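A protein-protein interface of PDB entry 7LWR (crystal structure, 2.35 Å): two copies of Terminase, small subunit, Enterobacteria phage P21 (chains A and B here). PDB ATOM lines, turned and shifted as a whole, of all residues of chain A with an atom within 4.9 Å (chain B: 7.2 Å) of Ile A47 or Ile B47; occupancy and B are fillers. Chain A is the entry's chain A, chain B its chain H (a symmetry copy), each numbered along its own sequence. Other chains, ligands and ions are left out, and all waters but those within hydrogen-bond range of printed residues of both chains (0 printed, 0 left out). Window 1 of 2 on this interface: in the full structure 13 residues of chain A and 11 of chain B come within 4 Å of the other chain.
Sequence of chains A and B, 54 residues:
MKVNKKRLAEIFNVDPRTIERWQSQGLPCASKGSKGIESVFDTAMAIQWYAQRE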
ATOM      1  N   ILE A  11       6.848  -0.288   1.121  1.00  0.00           N
ATOM      2  CA  ILE A  11       7.669   0.451   2.119  1.00  0.00           C
ATOM      3  C   ILE A  11       8.126   1.791   1.525  1.00  0.00           C
ATOM      4  O   ILE A  11       7.929   2.846   2.167  1.00  0.00           O
ATOM      5  CB  ILE A  11       8.821  -0.433   2.582  1.00  0.00           C
ATOM      6  CG1 ILE A  11       8.290  -1.620   3.389  1.00  0.00           C
ATOM      7  CG2 ILE A  11       9.850   0.386   3.347  1.00  0.00           C
ATOM      8  CD1 ILE A  11       9.284  -2.690   3.658  1.00  0.00           C
ATOM      9  N   PHE A  12       8.669   1.773   0.317  1.00  0.00           N
ATOM     10  CA  PHE A  12       9.029   3.016  -0.399  1.00  0.00           C
ATOM     11  C   PHE A  12       7.798   3.732  -0.957  1.00  0.00           C
ATOM     12  O   PHE A  12       7.901   4.859  -1.355  1.00  0.00           O
ATOM     13  CB  PHE A  12      10.068   2.736  -1.487  1.00  0.00           C
ATOM     14  CG  PHE A  12      11.428   2.413  -0.940  1.00  0.00           C
ATOM     15  CD1 PHE A  12      11.736   1.143  -0.507  1.00  0.00           C
ATOM     16  CD2 PHE A  12      12.386   3.390  -0.817  1.00  0.00           C
ATOM     17  CE1 PHE A  12      12.979   0.853   0.003  1.00  0.00           C
ATOM     18  CE2 PHE A  12      13.633   3.086  -0.294  1.00  0.00           C
ATOM     19  CZ  PHE A  12      13.928   1.818   0.089  1.00  0.00           C
ATOM     20  N   THR A  43      15.789  -4.834   3.390  1.00  0.00           N
ATOM     21  CA  THR A  43      15.284  -3.455   3.583  1.00  0.00           C
ATOM     22  C   THR A  43      16.371  -2.484   4.038  1.00  0.00           C
ATOM     23  O   THR A  43      16.306  -1.322   3.601  1.00  0.00           O
ATOM     24  CB  THR A  43      14.118  -3.344   4.554  1.00  0.00           C
ATOM     25  OG1 THR A  43      14.426  -3.863   5.831  1.00  0.00           O
ATOM     26  CG2 THR A  43      12.877  -3.998   4.010  1.00  0.00           C
ATOM     27  N   ALA A  44      17.278  -2.910   4.920  1.00  0.00           N
ATOM     28  CA  ALA A  44      18.382  -2.071   5.394  1.00  0.00           C
ATOM     29  C   ALA A  44      19.296  -1.761   4.218  1.00  0.00           C
ATOM     30  O   ALA A  44      19.664  -0.601   4.015  1.00  0.00           O
ATOM     31  CB  ALA A  44      19.123  -2.731   6.510  1.00  0.00           C
ATOM     32  N   MET A  45      19.637  -2.789   3.465  1.00  0.00           N
ATOM     33  CA  MET A  45      20.472  -2.672   2.258  1.00  0.00           C
ATOM     34  C   MET A  45      19.774  -1.735   1.302  1.00  0.00           C
ATOM     35  O   MET A  45      20.428  -0.857   0.775  1.00  0.00           O
ATOM     36  CB  MET A  45      20.705  -4.048   1.635  1.00  0.00           C
ATOM     37  CG  MET A  45      21.770  -4.929   2.350  1.00  0.00           C
ATOM     38  SD  MET A  45      23.473  -4.416   2.077  1.00  0.00           S
ATOM     39  CE  MET A  45      23.507  -4.602   0.292  1.00  0.00           C
ATOM     40  N   ALA A  46      18.474  -1.860   1.163  1.00  0.00           N
ATOM     41  CA  ALA A  46      17.687  -1.039   0.231  1.00  0.00           C
ATOM     42  C   ALA A  46      17.743   0.417   0.672  1.00  0.00           C
ATOM     43  O   ALA A  46      17.962   1.313  -0.172  1.00  0.00           O
ATOM     44  CB  ALA A  46      16.278  -1.547   0.162  1.00  0.00           C
ATOM     45  N   ILE A  47      17.532   0.659   1.951  1.00  0.00           N
ATOM     46  CA  ILE A  47      17.480   2.042   2.488  1.00  0.00           C
ATOM     47  C   ILE A  47      18.849   2.722   2.403  1.00  0.00           C
ATOM     48  O   ILE A  47      18.898   3.930   2.103  1.00  0.00           O
ATOM     49  CB  ILE A  47      16.888   2.028   3.893  1.00  0.00           C
ATOM     50  CG1 ILE A  47      15.392   1.731   3.843  1.00  0.00           C
ATOM     51  CG2 ILE A  47      17.169   3.345   4.586  1.00  0.00           C
ATOM     52  CD1 ILE A  47      14.813   1.210   5.135  1.00  0.00           C
ATOM     53  N   GLN A  48      19.930   2.024   2.682  1.00  0.00           N
ATOM     54  CA  GLN A  48      21.289   2.629   2.626  1.00  0.00           C
ATOM     55  C   GLN A  48      21.614   3.023   1.186  1.00  0.00           C
ATOM     56  O   GLN A  48      22.211   4.088   0.930  1.00  0.00           O
ATOM     57  CB  GLN A  48      22.335   1.701   3.219  1.00  0.00           C
ATOM     58  CG  GLN A  48      22.408   1.785   4.735  1.00  0.00           C
ATOM     59  CD  GLN A  48      23.396   0.854   5.388  1.00  0.00           C
ATOM     60  OE1 GLN A  48      24.601   1.085   5.305  1.00  0.00           O
ATOM     61  NE2 GLN A  48      22.878  -0.178   6.051  1.00  0.00           N
ATOM     62  N   TRP A  49      21.242   2.140   0.266  1.00  0.00           N
ATOM     63  CA  TRP A  49      21.462   2.340  -1.183  1.00  0.00           C
ATOM     64  C   TRP A  49      20.730   3.610  -1.604  1.00  0.00           C
ATOM     65  O   TRP A  49      21.361   4.512  -2.153  1.00  0.00           O
ATOM     66  CB  TRP A  49      20.999   1.119  -1.951  1.00  0.00           C
ATOM     67  CG  TRP A  49      21.121   1.293  -3.418  1.00  0.00           C
ATOM     68  CD1 TRP A  49      22.260   1.221  -4.145  1.00  0.00           C
ATOM     69  CD2 TRP A  49      20.081   1.688  -4.326  1.00  0.00           C
ATOM     70  NE1 TRP A  49      21.988   1.490  -5.458  1.00  0.00           N
ATOM     71  CE2 TRP A  49      20.663   1.785  -5.599  1.00  0.00           C
ATOM     72  CE3 TRP A  49      18.726   1.946  -4.191  1.00  0.00           C
ATOM     73  CZ2 TRP A  49      19.931   2.090  -6.737  1.00  0.00           C
ATOM     74  CZ3 TRP A  49      18.001   2.272  -5.310  1.00  0.00           C
ATOM     75  CH2 TRP A  49      18.593   2.356  -6.557  1.00  0.00           C
ATOM     76  N   TYR A  50      19.424   3.633  -1.375  1.00  0.00           N
ATOM     77  CA  TYR A  50      18.562   4.778  -1.761  1.00  0.00           C
ATOM     78  C   TYR A  50      19.141   6.074  -1.189  1.00  0.00           C
ATOM     79  O   TYR A  50      19.164   7.095  -1.905  1.00  0.00           O
ATOM     80  CB  TYR A  50      17.128   4.573  -1.281  1.00  0.00           C
ATOM     81  CG  TYR A  50      16.210   5.748  -1.456  1.00  0.00           C
ATOM     82  CD1 TYR A  50      15.463   5.896  -2.599  1.00  0.00           C
ATOM     83  CD2 TYR A  50      16.011   6.649  -0.438  1.00  0.00           C
ATOM     84  CE1 TYR A  50      14.603   6.964  -2.770  1.00  0.00           C
ATOM     85  CE2 TYR A  50      15.166   7.736  -0.597  1.00  0.00           C
ATOM     86  CZ  TYR A  50      14.435   7.885  -1.761  1.00  0.00           C
ATOM     87  OH  TYR A  50      13.572   8.910  -1.911  1.00  0.00           O
ATOM     88  N   ALA A  51      19.574   6.016   0.074  1.00  0.00           N
ATOM     89  CA  ALA A  51      20.054   7.174   0.833  1.00  0.00           C
ATOM     90  C   ALA A  51      21.415   7.624   0.303  1.00  0.00           C
ATOM     91  O   ALA A  51      21.731   8.805   0.496  1.00  0.00           O
ATOM     92  CB  ALA A  51      20.119   6.858   2.285  1.00  0.00           C
ATOM     93  N   LEU B   8       8.958  -0.623  12.188  1.00  0.00           N
ATOM     94  CA  LEU B   8       9.835   0.432  11.643  1.00  0.00           C
ATOM     95  C   LEU B   8      11.289   0.145  11.977  1.00  0.00           C
ATOM     96  O   LEU B   8      12.125   0.316  11.088  1.00  0.00           O
ATOM     97  CB  LEU B   8       9.452   1.798  12.198  1.00  0.00           C
ATOM     98  CG  LEU B   8      10.089   2.916  11.409  1.00  0.00           C
ATOM     99  CD1 LEU B   8       9.551   2.891   9.987  1.00  0.00           C
ATOM    100  CD2 LEU B   8       9.881   4.248  12.085  1.00  0.00           C
ATOM    101  N   ILE B  11      12.442  -2.718   9.944  1.00  0.00           N
ATOM    102  CA  ILE B  11      12.668  -2.305   8.540  1.00  0.00           C
ATOM    103  C   ILE B  11      14.053  -1.657   8.434  1.00  0.00           C
ATOM    104  O   ILE B  11      14.769  -1.999   7.472  1.00  0.00           O
ATOM    105  CB  ILE B  11      11.498  -1.455   8.025  1.00  0.00           C
ATOM    106  CG1 ILE B  11      10.217  -2.289   7.973  1.00  0.00           C
ATOM    107  CG2 ILE B  11      11.791  -0.834   6.676  1.00  0.00           C
ATOM    108  CD1 ILE B  11       8.968  -1.462   7.866  1.00  0.00           C
ATOM    109  N   PHE B  12      14.425  -0.762   9.348  1.00  0.00           N
ATOM    110  CA  PHE B  12      15.712  -0.032   9.257  1.00  0.00           C
ATOM    111  C   PHE B  12      16.893  -0.852   9.798  1.00  0.00           C
ATOM    112  O   PHE B  12      18.007  -0.474   9.620  1.00  0.00           O
ATOM    113  CB  PHE B  12      15.592   1.333   9.909  1.00  0.00           C
ATOM    114  CG  PHE B  12      14.917   2.391   9.103  1.00  0.00           C
ATOM    115  CD1 PHE B  12      13.568   2.339   8.935  1.00  0.00           C
ATOM    116  CD2 PHE B  12      15.600   3.433   8.546  1.00  0.00           C
ATOM    117  CE1 PHE B  12      12.911   3.304   8.203  1.00  0.00           C
ATOM    118  CE2 PHE B  12      14.931   4.402   7.840  1.00  0.00           C
ATOM    119  CZ  PHE B  12      13.588   4.353   7.688  1.00  0.00           C
ATOM    120  N   ASN B  13      16.629  -2.024  10.365  1.00  0.00           N
ATOM    121  CA  ASN B  13      17.576  -2.933  11.056  1.00  0.00           C
ATOM    122  C   ASN B  13      18.306  -2.166  12.159  1.00  0.00           C
ATOM    123  O   ASN B  13      19.522  -2.200  12.221  1.00  0.00           O
ATOM    124  CB  ASN B  13      18.507  -3.606  10.052  1.00  0.00           C
ATOM    125  CG  ASN B  13      19.174  -4.831  10.619  1.00  0.00           C
ATOM    126  OD1 ASN B  13      18.472  -5.706  11.113  1.00  0.00           O
ATOM    127  ND2 ASN B  13      20.499  -4.874  10.552  1.00  0.00           N
ATOM    128  N   TRP B  22      16.164   9.258  16.468  1.00  0.00           N
ATOM    129  CA  TRP B  22      15.734   9.907  15.205  1.00  0.00           C
ATOM    130  C   TRP B  22      14.525  10.811  15.423  1.00  0.00           C
ATOM    131  O   TRP B  22      14.432  11.812  14.776  1.00  0.00           O
ATOM    132  CB  TRP B  22      15.478   8.830  14.166  1.00  0.00           C
ATOM    133  CG  TRP B  22      16.735   8.163  13.738  1.00  0.00           C
ATOM    134  CD1 TRP B  22      18.011   8.558  13.993  1.00  0.00           C
ATOM    135  CD2 TRP B  22      16.831   7.024  12.893  1.00  0.00           C
ATOM    136  NE1 TRP B  22      18.887   7.712  13.382  1.00  0.00           N
ATOM    137  CE2 TRP B  22      18.180   6.769  12.704  1.00  0.00           C
ATOM    138  CE3 TRP B  22      15.900   6.211  12.254  1.00  0.00           C
ATOM    139  CZ2 TRP B  22      18.612   5.733  11.896  1.00  0.00           C
ATOM    140  CZ3 TRP B  22      16.321   5.174  11.448  1.00  0.00           C
ATOM    141  CH2 TRP B  22      17.673   4.917  11.318  1.00  0.00           C
ATOM    142  N   LEU B  27      12.430  13.082  12.776  1.00  0.00           N
ATOM    143  CA  LEU B  27      11.807  12.020  11.948  1.00  0.00           C
ATOM    144  C   LEU B  27      10.342  12.079  12.334  1.00  0.00           C
ATOM    145  O   LEU B  27      10.049  12.027  13.518  1.00  0.00           O
ATOM    146  CB  LEU B  27      12.426  10.631  12.142  1.00  0.00           C
ATOM    147  CG  LEU B  27      11.669   9.507  11.447  1.00  0.00           C
ATOM    148  CD1 LEU B  27      12.592   8.496  10.814  1.00  0.00           C
ATOM    149  CD2 LEU B  27      10.724   8.820  12.378  1.00  0.00           C
ATOM    150  N   ASP B  42       4.924   6.594   8.798  1.00  0.00           N
ATOM    151  CA  ASP B  42       4.901   6.326   7.329  1.00  0.00           C
ATOM    152  C   ASP B  42       6.314   5.967   6.866  1.00  0.00           C
ATOM    153  O   ASP B  42       7.191   6.839   6.974  1.00  0.00           O
ATOM    154  CB  ASP B  42       4.329   7.473   6.490  1.00  0.00           C
ATOM    155  CG  ASP B  42       4.335   7.188   4.995  1.00  0.00           C
ATOM    156  OD1 ASP B  42       3.401   6.522   4.509  1.00  0.00           O
ATOM    157  OD2 ASP B  42       5.262   7.596   4.345  1.00  0.00           O
ATOM    158  N   THR B  43       6.473   4.753   6.313  1.00  0.00           N
ATOM    159  CA  THR B  43       7.774   4.134   5.936  1.00  0.00           C
ATOM    160  C   THR B  43       8.498   4.935   4.854  1.00  0.00           C
ATOM    161  O   THR B  43       9.683   5.083   4.917  1.00  0.00           O
ATOM    162  CB  THR B  43       7.631   2.653   5.577  1.00  0.00           C
ATOM    163  OG1 THR B  43       6.667   2.440   4.542  1.00  0.00           O
ATOM    164  CG2 THR B  43       7.303   1.834   6.804  1.00  0.00           C
ATOM    165  N   ALA B  44       7.796   5.394   3.838  1.00  0.00           N
ATOM    166  CA  ALA B  44       8.411   6.203   2.772  1.00  0.00           C
ATOM    167  C   ALA B  44       8.854   7.525   3.399  1.00  0.00           C
ATOM    168  O   ALA B  44       9.932   7.996   3.113  1.00  0.00           O
ATOM    169  CB  ALA B  44       7.449   6.371   1.633  1.00  0.00           C
ATOM    170  N   MET B  45       8.023   8.076   4.253  1.00  0.00           N
ATOM    171  CA  MET B  45       8.313   9.331   4.991  1.00  0.00           C
ATOM    172  C   MET B  45       9.588   9.167   5.828  1.00  0.00           C
ATOM    173  O   MET B  45      10.422  10.043   5.811  1.00  0.00           O
ATOM    174  CB  MET B  45       7.132   9.643   5.896  1.00  0.00           C
ATOM    175  CG  MET B  45       7.076  11.039   6.278  1.00  0.00           C
ATOM    176  SD  MET B  45       5.864  11.794   5.306  1.00  0.00           S
ATOM    177  CE  MET B  45       6.150  13.469   5.860  1.00  0.00           C
ATOM    178  N   ALA B  46       9.716   8.065   6.550  1.00  0.00           N
ATOM    179  CA  ALA B  46      10.882   7.796   7.397  1.00  0.00           C
ATOM    180  C   ALA B  46      12.121   7.665   6.514  1.00  0.00           C
ATOM    181  O   ALA B  46      13.180   8.189   6.849  1.00  0.00           O
ATOM    182  CB  ALA B  46      10.638   6.559   8.192  1.00  0.00           C
ATOM    183  N   ILE B  47      11.979   6.954   5.423  1.00  0.00           N
ATOM    184  CA  ILE B  47      13.083   6.749   4.458  1.00  0.00           C
ATOM    185  C   ILE B  47      13.519   8.087   3.862  1.00  0.00           C
ATOM    186  O   ILE B  47      14.711   8.275   3.727  1.00  0.00           O
ATOM    187  CB  ILE B  47      12.690   5.695   3.410  1.00  0.00           C
ATOM    188  CG1 ILE B  47      12.634   4.319   4.064  1.00  0.00           C
ATOM    189  CG2 ILE B  47      13.640   5.757   2.230  1.00  0.00           C
ATOM    190  CD1 ILE B  47      12.144   3.237   3.176  1.00  0.00           C
ATOM    191  N   GLN B  48      12.583   8.995   3.575  1.00  0.00           N
ATOM    192  CA  GLN B  48      12.940  10.313   3.009  1.00  0.00           C
ATOM    193  C   GLN B  48      13.764  11.025   4.076  1.00  0.00           C
ATOM    194  O   GLN B  48      14.772  11.660   3.725  1.00  0.00           O
ATOM    195  CB  GLN B  48      11.697  11.056   2.529  1.00  0.00           C
ATOM    196  CG  GLN B  48      11.299  10.755   1.088  1.00  0.00           C
ATOM    197  CD  GLN B  48       9.971  11.378   0.720  1.00  0.00           C
ATOM    198  OE1 GLN B  48       8.953  10.701   0.570  1.00  0.00           O
ATOM    199  NE2 GLN B  48       9.999  12.688   0.547  1.00  0.00           N
ATOM    200  N   TRP B  49      13.343  10.904   5.334  1.00  0.00           N
ATOM    201  CA  TRP B  49      14.011  11.575   6.463  1.00  0.00           C
ATOM    202  C   TRP B  49      15.452  11.072   6.574  1.00  0.00           C
ATOM    203  O   TRP B  49      16.383  11.916   6.503  1.00  0.00           O
ATOM    204  CB  TRP B  49      13.274  11.363   7.769  1.00  0.00           C
ATOM    205  CG  TRP B  49      13.878  12.177   8.864  1.00  0.00           C
ATOM    206  CD1 TRP B  49      13.654  13.493   9.128  1.00  0.00           C
ATOM    207  CD2 TRP B  49      14.851  11.741   9.808  1.00  0.00           C
ATOM    208  NE1 TRP B  49      14.381  13.892  10.207  1.00  0.00           N
ATOM    209  CE2 TRP B  49      15.125  12.840  10.643  1.00  0.00           C
ATOM    210  CE3 TRP B  49      15.456  10.520  10.080  1.00  0.00           C
ATOM    211  CZ2 TRP B  49      16.020  12.757  11.699  1.00  0.00           C
ATOM    212  CZ3 TRP B  49      16.339  10.434  11.128  1.00  0.00           C
ATOM    213  CH2 TRP B  49      16.590  11.531  11.940  1.00  0.00           C
ATOM    214  N   TYR B  50      15.627   9.761   6.757  1.00  0.00           N
ATOM    215  CA  TYR B  50      16.955   9.105   6.784  1.00  0.00           C
ATOM    216  C   TYR B  50      17.811   9.586   5.601  1.00  0.00           C
ATOM    217  O   TYR B  50      19.002   9.842   5.832  1.00  0.00           O
ATOM    218  CB  TYR B  50      16.791   7.591   6.861  1.00  0.00           C
ATOM    219  CG  TYR B  50      18.078   6.827   6.870  1.00  0.00           C
ATOM    220  CD1 TYR B  50      18.724   6.483   5.691  1.00  0.00           C
ATOM    221  CD2 TYR B  50      18.647   6.437   8.065  1.00  0.00           C
ATOM    222  CE1 TYR B  50      19.938   5.829   5.711  1.00  0.00           C
ATOM    223  CE2 TYR B  50      19.820   5.717   8.091  1.00  0.00           C
ATOM    224  CZ  TYR B  50      20.470   5.428   6.910  1.00  0.00           C
ATOM    225  OH  TYR B  50      21.634   4.745   6.945  1.00  0.00           O
ATOM    226  N   ALA B  51      17.250   9.715   4.397  1.00  0.00           N
ATOM    227  CA  ALA B  51      17.985  10.042   3.157  1.00  0.00           C
ATOM    228  C   ALA B  51      18.478  11.505   3.127  1.00  0.00           C
ATOM    229  O   ALA B  51      19.563  11.744   2.505  1.00  0.00           O
ATOM    230  CB  ALA B  51      17.117   9.719   1.969  1.00  0.00           C
ATOM    231  N   GLN B  52      17.739  12.448   3.744  1.00  0.00           N
ATOM    232  CA  GLN B  52      18.083  13.890   3.802  1.00  0.00           C
ATOM    233  C   GLN B  52      19.326  14.107   4.667  1.00  0.00           C
ATOM    234  O   GLN B  52      20.168  14.936   4.261  1.00  0.00           O
ATOM    235  CB  GLN B  52      16.916  14.722   4.324  1.00  0.00           C
ATOM    236  CG  GLN B  52      17.245  16.202   4.491  1.00  0.00           C
ATOM    237  CD  GLN B  52      16.979  16.696   5.892  1.00  0.00           C
ATOM    238  OE1 GLN B  52      17.297  16.036   6.886  1.00  0.00           O
ATOM    239  NE2 GLN B  52      16.405  17.883   5.979  1.00  0.00           N
ATOM    240  N   GLU B  54      21.953  12.747   4.873  1.00  0.00           N
ATOM    241  CA  GLU B  54      23.123  12.675   3.954  1.00  0.00           C
ATOM    242  C   GLU B  54      22.695  13.120   2.555  1.00  0.00           C
ATOM    243  O   GLU B  54      22.920  14.290   2.235  1.00  0.00           O
ATOM    244  CB  GLU B  54      23.722  11.275   3.991  1.00  0.00           C
ATOM    245  CG  GLU B  54      22.836  10.201   3.419  1.00  0.00           C
ATOM    246  CD  GLU B  54      23.052   8.861   4.076  1.00  0.00           C
ATOM    247  OE1 GLU B  54      24.241   8.429   4.156  1.00  0.00           O
ATOM    248  OE2 GLU B  54      22.032   8.275   4.542  1.00  0.00           O
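O of Ile A11 sits at hydrogen-bond distance from N of Ala B44, at 3.0 Å. O of Ile B11 sits at hydrogen-bond distance from OG1 of Thr A43, at 2.5 Å. O of Ile A11 is in hydrogen-bond range of OG1 of Thr B43, 2.7 Å away.
The backbone NH (N) of Ala B44 lies within hydrogen-bond range of the side-chain carboxylate (OD2) of Asp B42 (3.4 Å).
Among the printed residues, merely in contact across the chains: Ala A51 with Glu B54, Phe A12 with Ala B44, Ala A51 with Tyr B50, Ile A47 with Ile B47, Ile A11 with Ile B47, Ile A47 with Tyr B50, Phe A12 with Ile B47, Tyr A50 with Ile B47, Ala A44 with Ile B11, Ala A44 with Asn B13, Gln A48 with Tyr B50, Tyr A50 with Ala B51, Ala A51 with Ala B51 and Ile A47 with Ile B11.
Ile A47 touches three residues of chain B. Ile B47 touches just these residues of chain A: Ile A11, Phe A12, Ile A47 and Tyr A50. Of the printed residues of chain A, Tyr B50 touches Ile A47 (3.7 Å), Gln A48 (3.8 Å) and Ala A51 (3.6 Å). Of the printed residues of chain A, Ala B44 touches Ile A11 (3.0 Å) and Phe A12 (3.4 Å). Printed residues of chain B within 4 Å of Ala A51: Tyr B50, Ala B51 and Glu B54. Trp B49 touches none of the printed residues of chain A. Trp A49 touches none of the printed residues of chain B. The nearest residue of chain B that does not touch Ile A47 is Phe B12 (4.1 Å).
Hydrophobic or aromatic side chains of chain A within 4 Å of the printed part of chain B: Ile A11, Phe A12, Ala A44, Ile A47, Tyr A50 and Ala A51. Printed residues of chain B that touch a printed residue of chain A: Ile B11, Asn B13, Thr B43, Ala B44, Ile B47, Tyr B50, Ala B51 and Glu B54. Hydrophobic or aromatic side chains of chain B that line the printed part of chain A: Ile B11, Ala B44, Ile B47, Tyr B50 and Ala B51. Among the printed residues, 17 pairs touch across the chains. Among the printed residues, no Asp or Glu carboxylate lies within 4 Å of a Lys or Arg side-chain nitrogen of the other chain.
Ile A11 touches Ile B47, and with the chains exchanged Ile A47 touches Ile B11. Ile B47 touches its own counterpart, Ile A47. Gln A48 touches Tyr B50, but with the chains exchanged Tyr A50 does not touch Gln B48 (4.2 Å). Tyr A50 touches Ala B51, and with the chains exchanged Ala A51 touches Tyr B50. Positions printed for both chains: 11, 12, 43, 44, 45, 46, 47, 48, 49, 50 and 51.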
